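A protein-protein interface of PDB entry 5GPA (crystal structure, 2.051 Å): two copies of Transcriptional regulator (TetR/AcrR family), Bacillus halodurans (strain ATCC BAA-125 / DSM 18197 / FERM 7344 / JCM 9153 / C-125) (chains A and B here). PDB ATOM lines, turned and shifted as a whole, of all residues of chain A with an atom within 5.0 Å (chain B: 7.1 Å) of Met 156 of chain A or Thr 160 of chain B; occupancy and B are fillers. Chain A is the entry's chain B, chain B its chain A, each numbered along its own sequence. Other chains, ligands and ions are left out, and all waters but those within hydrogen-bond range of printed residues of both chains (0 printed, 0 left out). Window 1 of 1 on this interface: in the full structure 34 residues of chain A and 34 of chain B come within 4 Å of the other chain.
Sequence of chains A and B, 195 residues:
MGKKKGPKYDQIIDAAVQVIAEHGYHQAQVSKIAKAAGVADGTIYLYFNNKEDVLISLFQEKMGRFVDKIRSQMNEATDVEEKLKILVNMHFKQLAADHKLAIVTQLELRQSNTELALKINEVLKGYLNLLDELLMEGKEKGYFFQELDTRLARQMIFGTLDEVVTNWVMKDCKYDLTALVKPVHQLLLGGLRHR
The backbone carbonyl oxygen of Met 156 of chain A sits at hydrogen-bond distance from the side-chain hydroxyl of Thr 160 of chain A. OG1 of Thr 160 of chain B lies within hydrogen-bond range of O of Met 156 of chain B.
The side-chain hydroxyl (OG1) of Thr 160 of chain B sits close to the side-chain hydroxyl (OG1) of Thr 160 of chain A, 3.5 Å away. O of Leu 188 of chain A lies within hydrogen-bond range of N of Leu 192 of chain B, at 2.9 Å.
Hydrophobic or aromatic side chains of chain B within 4 Å of the printed part of chain A: Met 156, Val 164, Val 184, Leu 187 and Leu 192. Hydrophobic or aromatic side chains of chain A that line the printed part of chain B: Leu 152, Ala 153, Met 156, Ile 157 and Phe 158. Among the printed residues, 17 pairs touch across the chains. Among the printed residues, no Asp or Glu carboxylate lies within 4 Å of a Lys or Arg side-chain nitrogen of the other chain.
Leu 152 of chain A touches Val 184 of chain B (CD2 to CG2, 3.8 Å). Leu 152 of chain A touches Leu 187 of chain B. Ala 153 of chain A touches Leu 192 of chain B. Val 164 of chain B touches Gln 155 of chain A. CG of Met 156 of chain A touches OG1 of Thr 160 of chain B, 3.3 Å away. SD of Met 156 of chain A touches CG of Leu 187 of chain B, at 3.7 Å. CE of Met 156 of chain A touches CD2 of Leu 192 of chain B, at 3.8 Å. Ile 157 of chain A touches Leu 192 of chain B (CD1 to CD1, 3.99 Å). Gly 159 of chain A touches Gly 159 of chain B (CA to O, 3.6 Å). OG1 of Thr 160 of chain A touches CG of Met 156 of chain B, at 3.3 Å.
Met 156 of chain A touches three residues of chain B. Thr 160 of chain B touches just these residues of chain A: Met 156 (3.3 Å) and Thr 160 (3.5 Å). Printed residues of chain B within 4 Å of Gln 155 of chain A: Glu 163 (3.5 Å) and Val 164 (3.6 Å). Printed residues of chain A within 4 Å of Leu 192 of chain B: Ala 153 (3.9 Å), Met 156 (3.8 Å), Ile 157 (3.99 Å) and Leu 188 (2.9 Å). Printed residues of chain A within 4 Å of Met 156 of chain B: Thr 160. Of the printed residues of chain A, Gly 159 of chain B touches Gly 159 (3.6 Å). The nearest residue of chain B that does not touch Met 156 of chain A is Met 156 of chain B (4.5 Å).
Met 156 of chain A touches Thr 160 of chain B, and with the chains exchanged Thr 160 of chain A touches Met 156 of chain B. Gly 159 of chain B touches its own counterpart, Gly 159 of chain A. Thr 160 of chain B touches its own counterpart, Thr 160 of chain A. Of the 17 pairs that touch across the chains among the printed residues, 4 have their exchanged pair printed and touching as well.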
ATOM      1  N   LEU A 152      27.780 -23.991 -26.854  1.00  0.00           N
ATOM      2  CA  LEU A 152      27.449 -22.596 -27.125  1.00  0.00           C
ATOM      3  C   LEU A 152      27.103 -22.389 -28.597  1.00  0.00           C
ATOM      4  O   LEU A 152      26.190 -21.634 -28.915  1.00  0.00           O
ATOM      5  CB  LEU A 152      28.608 -21.671 -26.745  1.00  0.00           C
ATOM      6  CG  LEU A 152      28.807 -21.256 -25.288  1.00  0.00           C
ATOM      7  CD1 LEU A 152      29.979 -20.235 -25.220  1.00  0.00           C
ATOM      8  CD2 LEU A 152      27.528 -20.665 -24.686  1.00  0.00           C
ATOM      9  N   ALA A 153      27.834 -23.047 -29.488  1.00  0.00           N
ATOM     10  CA  ALA A 153      27.568 -22.896 -30.911  1.00  0.00           C
ATOM     11  C   ALA A 153      26.193 -23.493 -31.253  1.00  0.00           C
ATOM     12  O   ALA A 153      25.443 -22.937 -32.059  1.00  0.00           O
ATOM     13  CB  ALA A 153      28.639 -23.543 -31.734  1.00  0.00           C
ATOM     14  N   ARG A 154      25.879 -24.618 -30.627  1.00  0.00           N
ATOM     15  CA  ARG A 154      24.592 -25.266 -30.827  1.00  0.00           C
ATOM     16  C   ARG A 154      23.472 -24.328 -30.407  1.00  0.00           C
ATOM     17  O   ARG A 154      22.459 -24.189 -31.099  1.00  0.00           O
ATOM     18  CB  ARG A 154      24.522 -26.562 -30.034  1.00  0.00           C
ATOM     19  CG  ARG A 154      23.149 -27.219 -30.108  1.00  0.00           C
ATOM     20  CD  ARG A 154      23.163 -28.517 -29.336  1.00  0.00           C
ATOM     21  NE  ARG A 154      22.779 -28.304 -27.969  1.00  0.00           N
ATOM     22  CZ  ARG A 154      22.706 -29.261 -27.050  1.00  0.00           C
ATOM     23  NH1 ARG A 154      23.041 -30.527 -27.338  1.00  0.00           N
ATOM     24  NH2 ARG A 154      22.296 -28.940 -25.834  1.00  0.00           N
ATOM     25  N   GLN A 155      23.657 -23.680 -29.268  1.00  0.00           N
ATOM     26  CA  GLN A 155      22.658 -22.755 -28.746  1.00  0.00           C
ATOM     27  C   GLN A 155      22.541 -21.506 -29.609  1.00  0.00           C
ATOM     28  O   GLN A 155      21.437 -20.988 -29.800  1.00  0.00           O
ATOM     29  CB  GLN A 155      22.965 -22.400 -27.280  1.00  0.00           C
ATOM     30  CG  GLN A 155      22.753 -23.639 -26.375  1.00  0.00           C
ATOM     31  CD  GLN A 155      23.227 -23.426 -24.951  1.00  0.00           C
ATOM     32  OE1 GLN A 155      23.931 -22.473 -24.652  1.00  0.00           O
ATOM     33  NE2 GLN A 155      22.824 -24.314 -24.061  1.00  0.00           N
ATOM     34  N   MET A 156      23.658 -21.032 -30.155  1.00  0.00           N
ATOM     35  CA  MET A 156      23.595 -19.946 -31.139  1.00  0.00           C
ATOM     36  C   MET A 156      22.806 -20.307 -32.406  1.00  0.00           C
ATOM     37  O   MET A 156      21.964 -19.533 -32.870  1.00  0.00           O
ATOM     38  CB  MET A 156      24.994 -19.499 -31.553  1.00  0.00           C
ATOM     39  CG  MET A 156      24.977 -18.332 -32.546  1.00  0.00           C
ATOM     40  SD  MET A 156      26.627 -17.802 -33.101  1.00  0.00           S
ATOM     41  CE  MET A 156      27.055 -19.171 -34.181  1.00  0.00           C
ATOM     42  N   ILE A 157      23.117 -21.446 -32.996  1.00  0.00           N
ATOM     43  CA  ILE A 157      22.460 -21.826 -34.226  1.00  0.00           C
ATOM     44  C   ILE A 157      20.979 -22.042 -33.952  1.00  0.00           C
ATOM     45  O   ILE A 157      20.144 -21.451 -34.618  1.00  0.00           O
ATOM     46  CB  ILE A 157      23.082 -23.085 -34.824  1.00  0.00           C
ATOM     47  CG1 ILE A 157      24.511 -22.756 -35.308  1.00  0.00           C
ATOM     48  CG2 ILE A 157      22.203 -23.659 -35.977  1.00  0.00           C
ATOM     49  CD1 ILE A 157      25.329 -24.008 -35.613  1.00  0.00           C
ATOM     50  N   PHE A 158      20.661 -22.856 -32.956  1.00  0.00           N
ATOM     51  CA  PHE A 158      19.265 -23.125 -32.673  1.00  0.00           C
ATOM     52  C   PHE A 158      18.509 -21.885 -32.193  1.00  0.00           C
ATOM     53  O   PHE A 158      17.376 -21.642 -32.638  1.00  0.00           O
ATOM     54  CB  PHE A 158      19.069 -24.233 -31.636  1.00  0.00           C
ATOM     55  CG  PHE A 158      17.619 -24.476 -31.353  1.00  0.00           C
ATOM     56  CD1 PHE A 158      16.847 -25.231 -32.239  1.00  0.00           C
ATOM     57  CD2 PHE A 158      17.002 -23.892 -30.250  1.00  0.00           C
ATOM     58  CE1 PHE A 158      15.482 -25.422 -32.005  1.00  0.00           C
ATOM     59  CE2 PHE A 158      15.646 -24.079 -30.017  1.00  0.00           C
ATOM     60  CZ  PHE A 158      14.891 -24.845 -30.897  1.00  0.00           C
ATOM     61  N   GLY A 159      19.111 -21.124 -31.282  1.00  0.00           N
ATOM     62  CA  GLY A 159      18.501 -19.910 -30.764  1.00  0.00           C
ATOM     63  C   GLY A 159      18.213 -18.906 -31.888  1.00  0.00           C
ATOM     64  O   GLY A 159      17.171 -18.256 -31.911  1.00  0.00           O
ATOM     65  N   THR A 160      19.135 -18.788 -32.833  1.00  0.00           N
ATOM     66  CA  THR A 160      18.978 -17.862 -33.945  1.00  0.00           C
ATOM     67  C   THR A 160      17.878 -18.334 -34.893  1.00  0.00           C
ATOM     68  O   THR A 160      17.009 -17.558 -35.257  1.00  0.00           O
ATOM     69  CB  THR A 160      20.309 -17.687 -34.734  1.00  0.00           C
ATOM     70  OG1 THR A 160      21.282 -17.045 -33.890  1.00  0.00           O
ATOM     71  CG2 THR A 160      20.093 -16.847 -36.016  1.00  0.00           C
ATOM     72  N   LEU A 161      17.918 -19.601 -35.292  1.00  0.00           N
ATOM     73  CA  LEU A 161      16.898 -20.129 -36.210  1.00  0.00           C
ATOM     74  C   LEU A 161      15.496 -19.989 -35.628  1.00  0.00           C
ATOM     75  O   LEU A 161      14.557 -19.598 -36.328  1.00  0.00           O
ATOM     76  CB  LEU A 161      17.161 -21.602 -36.526  1.00  0.00           C
ATOM     77  CG  LEU A 161      18.443 -21.905 -37.298  1.00  0.00           C
ATOM     78  CD1 LEU A 161      18.508 -23.388 -37.625  1.00  0.00           C
ATOM     79  CD2 LEU A 161      18.519 -21.073 -38.573  1.00  0.00           C
ATOM     80  N   LEU A 188      25.655 -16.977 -39.415  1.00  0.00           N
ATOM     81  CA  LEU A 188      26.133 -17.958 -38.438  1.00  0.00           C
ATOM     82  C   LEU A 188      27.608 -18.356 -38.685  1.00  0.00           C
ATOM     83  O   LEU A 188      28.374 -18.522 -37.733  1.00  0.00           O
ATOM     84  CB  LEU A 188      25.250 -19.203 -38.476  1.00  0.00           C
ATOM     85  CG  LEU A 188      23.781 -19.016 -38.046  1.00  0.00           C
ATOM     86  CD1 LEU A 188      23.011 -20.294 -38.356  1.00  0.00           C
ATOM     87  CD2 LEU A 188      23.673 -18.669 -36.565  1.00  0.00           C
ATOM     88  N   PHE B  92      23.789 -11.097 -18.914  1.00  0.00           N
ATOM     89  CA  PHE B  92      24.004 -12.260 -18.072  1.00  0.00           C
ATOM     90  C   PHE B  92      24.055 -11.885 -16.579  1.00  0.00           C
ATOM     91  O   PHE B  92      23.490 -12.591 -15.745  1.00  0.00           O
ATOM     92  CB  PHE B  92      25.291 -12.986 -18.483  1.00  0.00           C
ATOM     93  CG  PHE B  92      25.195 -13.706 -19.815  1.00  0.00           C
ATOM     94  CD1 PHE B  92      23.995 -13.741 -20.517  1.00  0.00           C
ATOM     95  CD2 PHE B  92      26.298 -14.345 -20.350  1.00  0.00           C
ATOM     96  CE1 PHE B  92      23.893 -14.401 -21.721  1.00  0.00           C
ATOM     97  CE2 PHE B  92      26.208 -15.010 -21.558  1.00  0.00           C
ATOM     98  CZ  PHE B  92      25.002 -15.027 -22.250  1.00  0.00           C
ATOM     99  N   ARG B 154      20.210  -8.606 -35.066  1.00  0.00           N
ATOM    100  CA  ARG B 154      19.493  -8.404 -33.806  1.00  0.00           C
ATOM    101  C   ARG B 154      18.848  -9.698 -33.337  1.00  0.00           C
ATOM    102  O   ARG B 154      18.880 -10.040 -32.148  1.00  0.00           O
ATOM    103  CB  ARG B 154      18.420  -7.310 -33.966  1.00  0.00           C
ATOM    104  CG  ARG B 154      17.387  -7.271 -32.849  1.00  0.00           C
ATOM    105  CD  ARG B 154      15.958  -7.026 -33.391  1.00  0.00           C
ATOM    106  NE  ARG B 154      15.939  -5.885 -34.300  1.00  0.00           N
ATOM    107  CZ  ARG B 154      15.024  -5.680 -35.242  1.00  0.00           C
ATOM    108  NH1 ARG B 154      14.026  -6.547 -35.403  1.00  0.00           N
ATOM    109  NH2 ARG B 154      15.119  -4.609 -36.022  1.00  0.00           N
ATOM    110  N   GLN B 155      18.272 -10.428 -34.287  1.00  0.00           N
ATOM    111  CA  GLN B 155      17.635 -11.695 -33.980  1.00  0.00           C
ATOM    112  C   GLN B 155      18.675 -12.736 -33.572  1.00  0.00           C
ATOM    113  O   GLN B 155      18.465 -13.504 -32.624  1.00  0.00           O
ATOM    114  CB  GLN B 155      16.793 -12.154 -35.184  1.00  0.00           C
ATOM    115  CG  GLN B 155      15.495 -11.289 -35.330  1.00  0.00           C
ATOM    116  CD  GLN B 155      14.751 -11.509 -36.646  1.00  0.00           C
ATOM    117  OE1 GLN B 155      15.250 -12.166 -37.538  1.00  0.00           O
ATOM    118  NE2 GLN B 155      13.586 -10.900 -36.781  1.00  0.00           N
ATOM    119  N   MET B 156      19.805 -12.760 -34.266  1.00  0.00           N
ATOM    120  CA  MET B 156      20.903 -13.644 -33.839  1.00  0.00           C
ATOM    121  C   MET B 156      21.378 -13.301 -32.428  1.00  0.00           C
ATOM    122  O   MET B 156      21.510 -14.175 -31.578  1.00  0.00           O
ATOM    123  CB  MET B 156      22.085 -13.562 -34.794  1.00  0.00           C
ATOM    124  CG  MET B 156      23.302 -14.420 -34.281  1.00  0.00           C
ATOM    125  SD  MET B 156      24.666 -14.511 -35.469  1.00  0.00           S
ATOM    126  CE  MET B 156      25.228 -12.857 -35.220  1.00  0.00           C
ATOM    127  N   ILE B 157      21.652 -12.026 -32.172  1.00  0.00           N
ATOM    128  CA  ILE B 157      22.152 -11.664 -30.859  1.00  0.00           C
ATOM    129  C   ILE B 157      21.121 -11.996 -29.776  1.00  0.00           C
ATOM    130  O   ILE B 157      21.430 -12.720 -28.824  1.00  0.00           O
ATOM    131  CB  ILE B 157      22.533 -10.175 -30.764  1.00  0.00           C
ATOM    132  CG1 ILE B 157      23.735  -9.865 -31.663  1.00  0.00           C
ATOM    133  CG2 ILE B 157      22.897  -9.805 -29.309  1.00  0.00           C
ATOM    134  CD1 ILE B 157      23.967  -8.381 -31.860  1.00  0.00           C
ATOM    135  N   PHE B 158      19.897 -11.484 -29.909  1.00  0.00           N
ATOM    136  CA  PHE B 158      18.911 -11.751 -28.880  1.00  0.00           C
ATOM    137  C   PHE B 158      18.596 -13.225 -28.775  1.00  0.00           C
ATOM    138  O   PHE B 158      18.506 -13.755 -27.675  1.00  0.00           O
ATOM    139  CB  PHE B 158      17.594 -10.998 -29.114  1.00  0.00           C
ATOM    140  CG  PHE B 158      16.575 -11.316 -28.068  1.00  0.00           C
ATOM    141  CD1 PHE B 158      16.704 -10.790 -26.778  1.00  0.00           C
ATOM    142  CD2 PHE B 158      15.545 -12.213 -28.329  1.00  0.00           C
ATOM    143  CE1 PHE B 158      15.791 -11.116 -25.789  1.00  0.00           C
ATOM    144  CE2 PHE B 158      14.632 -12.538 -27.335  1.00  0.00           C
ATOM    145  CZ  PHE B 158      14.759 -11.995 -26.079  1.00  0.00           C
ATOM    146  N   GLY B 159      18.394 -13.889 -29.911  1.00  0.00           N
ATOM    147  CA  GLY B 159      18.045 -15.297 -29.885  1.00  0.00           C
ATOM    148  C   GLY B 159      19.133 -16.136 -29.202  1.00  0.00           C
ATOM    149  O   GLY B 159      18.846 -17.110 -28.516  1.00  0.00           O
ATOM    150  N   THR B 160      20.394 -15.779 -29.409  1.00  0.00           N
ATOM    151  CA  THR B 160      21.495 -16.537 -28.772  1.00  0.00           C
ATOM    152  C   THR B 160      21.563 -16.296 -27.254  1.00  0.00           C
ATOM    153  O   THR B 160      21.630 -17.245 -26.485  1.00  0.00           O
ATOM    154  CB  THR B 160      22.862 -16.173 -29.407  1.00  0.00           C
ATOM    155  OG1 THR B 160      22.840 -16.523 -30.800  1.00  0.00           O
ATOM    156  CG2 THR B 160      24.013 -16.950 -28.709  1.00  0.00           C
ATOM    157  N   LEU B 161      21.552 -15.032 -26.826  1.00  0.00           N
ATOM    158  CA  LEU B 161      21.616 -14.702 -25.399  1.00  0.00           C
ATOM    159  C   LEU B 161      20.453 -15.347 -24.654  1.00  0.00           C
ATOM    160  O   LEU B 161      20.620 -15.934 -23.583  1.00  0.00           O
ATOM    161  CB  LEU B 161      21.579 -13.198 -25.191  1.00  0.00           C
ATOM    162  CG  LEU B 161      22.770 -12.423 -25.770  1.00  0.00           C
ATOM    163  CD1 LEU B 161      22.589 -10.930 -25.477  1.00  0.00           C
ATOM    164  CD2 LEU B 161      24.050 -12.951 -25.163  1.00  0.00           C
ATOM    165  N   ASP B 162      19.271 -15.267 -25.255  1.00  0.00           N
ATOM    166  CA  ASP B 162      18.075 -15.826 -24.642  1.00  0.00           C
ATOM    167  C   ASP B 162      18.118 -17.353 -24.531  1.00  0.00           C
ATOM    168  O   ASP B 162      17.700 -17.930 -23.527  1.00  0.00           O
ATOM    169  CB  ASP B 162      16.842 -15.382 -25.431  1.00  0.00           C
ATOM    170  CG  ASP B 162      15.577 -15.489 -24.613  1.00  0.00           C
ATOM    171  OD1 ASP B 162      15.518 -14.875 -23.517  1.00  0.00           O
ATOM    172  OD2 ASP B 162      14.666 -16.206 -25.060  1.00  0.00           O
ATOM    173  N   GLU B 163      18.636 -18.017 -25.559  1.00  0.00           N
ATOM    174  CA  GLU B 163      18.777 -19.456 -25.542  1.00  0.00           C
ATOM    175  C   GLU B 163      19.810 -19.912 -24.491  1.00  0.00           C
ATOM    176  O   GLU B 163      19.625 -20.931 -23.828  1.00  0.00           O
ATOM    177  CB  GLU B 163      19.185 -19.952 -26.938  1.00  0.00           C
ATOM    178  CG  GLU B 163      19.328 -21.452 -27.054  1.00  0.00           C
ATOM    179  CD  GLU B 163      17.979 -22.183 -26.990  1.00  0.00           C
ATOM    180  OE1 GLU B 163      16.926 -21.521 -27.088  1.00  0.00           O
ATOM    181  OE2 GLU B 163      17.974 -23.419 -26.828  1.00  0.00           O
ATOM    182  N   VAL B 164      20.895 -19.157 -24.344  1.00  0.00           N
ATOM    183  CA  VAL B 164      21.909 -19.491 -23.331  1.00  0.00           C
ATOM    184  C   VAL B 164      21.284 -19.368 -21.940  1.00  0.00           C
ATOM    185  O   VAL B 164      21.404 -20.263 -21.113  1.00  0.00           O
ATOM    186  CB  VAL B 164      23.159 -18.593 -23.449  1.00  0.00           C
ATOM    187  CG1 VAL B 164      24.100 -18.833 -22.253  1.00  0.00           C
ATOM    188  CG2 VAL B 164      23.891 -18.863 -24.782  1.00  0.00           C
ATOM    189  N   VAL B 165      20.595 -18.261 -21.693  1.00  0.00           N
ATOM    190  CA  VAL B 165      19.950 -18.043 -20.394  1.00  0.00           C
ATOM    191  C   VAL B 165      18.888 -19.082 -20.094  1.00  0.00           C
ATOM    192  O   VAL B 165      18.784 -19.575 -18.968  1.00  0.00           O
ATOM    193  CB  VAL B 165      19.297 -16.643 -20.309  1.00  0.00           C
ATOM    194  CG1 VAL B 165      18.530 -16.495 -18.986  1.00  0.00           C
ATOM    195  CG2 VAL B 165      20.366 -15.578 -20.444  1.00  0.00           C
ATOM    196  N   THR B 166      18.076 -19.403 -21.089  1.00  0.00           N
ATOM    197  CA  THR B 166      17.010 -20.370 -20.875  1.00  0.00           C
ATOM    198  C   THR B 166      17.559 -21.756 -20.532  1.00  0.00           C
ATOM    199  O   THR B 166      17.000 -22.465 -19.687  1.00  0.00           O
ATOM    200  CB  THR B 166      16.098 -20.426 -22.087  1.00  0.00           C
ATOM    201  OG1 THR B 166      15.407 -19.168 -22.169  1.00  0.00           O
ATOM    202  CG2 THR B 166      15.088 -21.550 -21.968  1.00  0.00           C
ATOM    203  N   VAL B 184      30.636 -16.202 -25.578  1.00  0.00           N
ATOM    204  CA  VAL B 184      29.426 -15.813 -26.330  1.00  0.00           C
ATOM    205  C   VAL B 184      29.721 -14.593 -27.175  1.00  0.00           C
ATOM    206  O   VAL B 184      29.444 -14.566 -28.372  1.00  0.00           O
ATOM    207  CB  VAL B 184      28.236 -15.523 -25.410  1.00  0.00           C
ATOM    208  CG1 VAL B 184      27.145 -14.748 -26.168  1.00  0.00           C
ATOM    209  CG2 VAL B 184      27.658 -16.837 -24.889  1.00  0.00           C
ATOM    210  N   LEU B 187      31.842 -15.494 -30.095  1.00  0.00           N
ATOM    211  CA  LEU B 187      31.089 -16.293 -31.044  1.00  0.00           C
ATOM    212  C   LEU B 187      30.163 -15.400 -31.892  1.00  0.00           C
ATOM    213  O   LEU B 187      30.054 -15.578 -33.096  1.00  0.00           O
ATOM    214  CB  LEU B 187      30.301 -17.377 -30.283  1.00  0.00           C
ATOM    215  CG  LEU B 187      29.625 -18.551 -31.000  1.00  0.00           C
ATOM    216  CD1 LEU B 187      30.541 -19.254 -31.984  1.00  0.00           C
ATOM    217  CD2 LEU B 187      29.115 -19.545 -29.955  1.00  0.00           C
ATOM    218  N   LEU B 188      29.538 -14.413 -31.270  1.00  0.00           N
ATOM    219  CA  LEU B 188      28.700 -13.472 -32.005  1.00  0.00           C
ATOM    220  C   LEU B 188      29.528 -12.684 -33.041  1.00  0.00           C
ATOM    221  O   LEU B 188      29.097 -12.453 -34.171  1.00  0.00           O
ATOM    222  CB  LEU B 188      28.017 -12.510 -31.036  1.00  0.00           C
ATOM    223  CG  LEU B 188      26.926 -13.181 -30.181  1.00  0.00           C
ATOM    224  CD1 LEU B 188      26.356 -12.261 -29.108  1.00  0.00           C
ATOM    225  CD2 LEU B 188      25.812 -13.700 -31.078  1.00  0.00           C
ATOM    226  N   LEU B 189      30.729 -12.287 -32.650  1.00  0.00           N
ATOM    227  CA  LEU B 189      31.588 -11.502 -33.532  1.00  0.00           C
ATOM    228  C   LEU B 189      32.197 -12.288 -34.682  1.00  0.00           C
ATOM    229  O   LEU B 189      32.314 -11.771 -35.785  1.00  0.00           O
ATOM    230  CB  LEU B 189      32.707 -10.866 -32.702  1.00  0.00           C
ATOM    231  CG  LEU B 189      32.289  -9.704 -31.796  1.00  0.00           C
ATOM    232  CD1 LEU B 189      33.489  -9.276 -30.927  1.00  0.00           C
ATOM    233  CD2 LEU B 189      31.806  -8.534 -32.631  1.00  0.00           C
ATOM    234  N   GLY B 190      32.580 -13.536 -34.432  1.00  0.00           N
ATOM    235  CA  GLY B 190      33.336 -14.314 -35.409  1.00  0.00           C
ATOM    236  C   GLY B 190      32.618 -15.520 -35.998  1.00  0.00           C
ATOM    237  O   GLY B 190      33.156 -16.215 -36.877  1.00  0.00           O
ATOM    238  N   GLY B 191      31.393 -15.768 -35.535  1.00  0.00           N
ATOM    239  CA  GLY B 191      30.634 -16.908 -36.031  1.00  0.00           C
ATOM    240  C   GLY B 191      31.327 -18.240 -35.817  1.00  0.00           C
ATOM    241  O   GLY B 191      32.242 -18.366 -34.989  1.00  0.00           O
ATOM    242  N   LEU B 192      30.889 -19.253 -36.555  1.00  0.00           N
ATOM    243  CA  LEU B 192      31.515 -20.571 -36.469  1.00  0.00           C
ATOM    244  C   LEU B 192      32.961 -20.596 -37.009  1.00  0.00           C
ATOM    245  O   LEU B 192      33.769 -21.405 -36.585  1.00  0.00           O
ATOM    246  CB  LEU B 192      30.684 -21.581 -37.243  1.00  0.00           C
ATOM    247  CG  LEU B 192      29.220 -21.756 -36.789  1.00  0.00           C
ATOM    248  CD1 LEU B 192      28.572 -22.829 -37.626  1.00  0.00           C
ATOM    249  CD2 LEU B 192      29.154 -22.122 -35.313  1.00  0.00           C
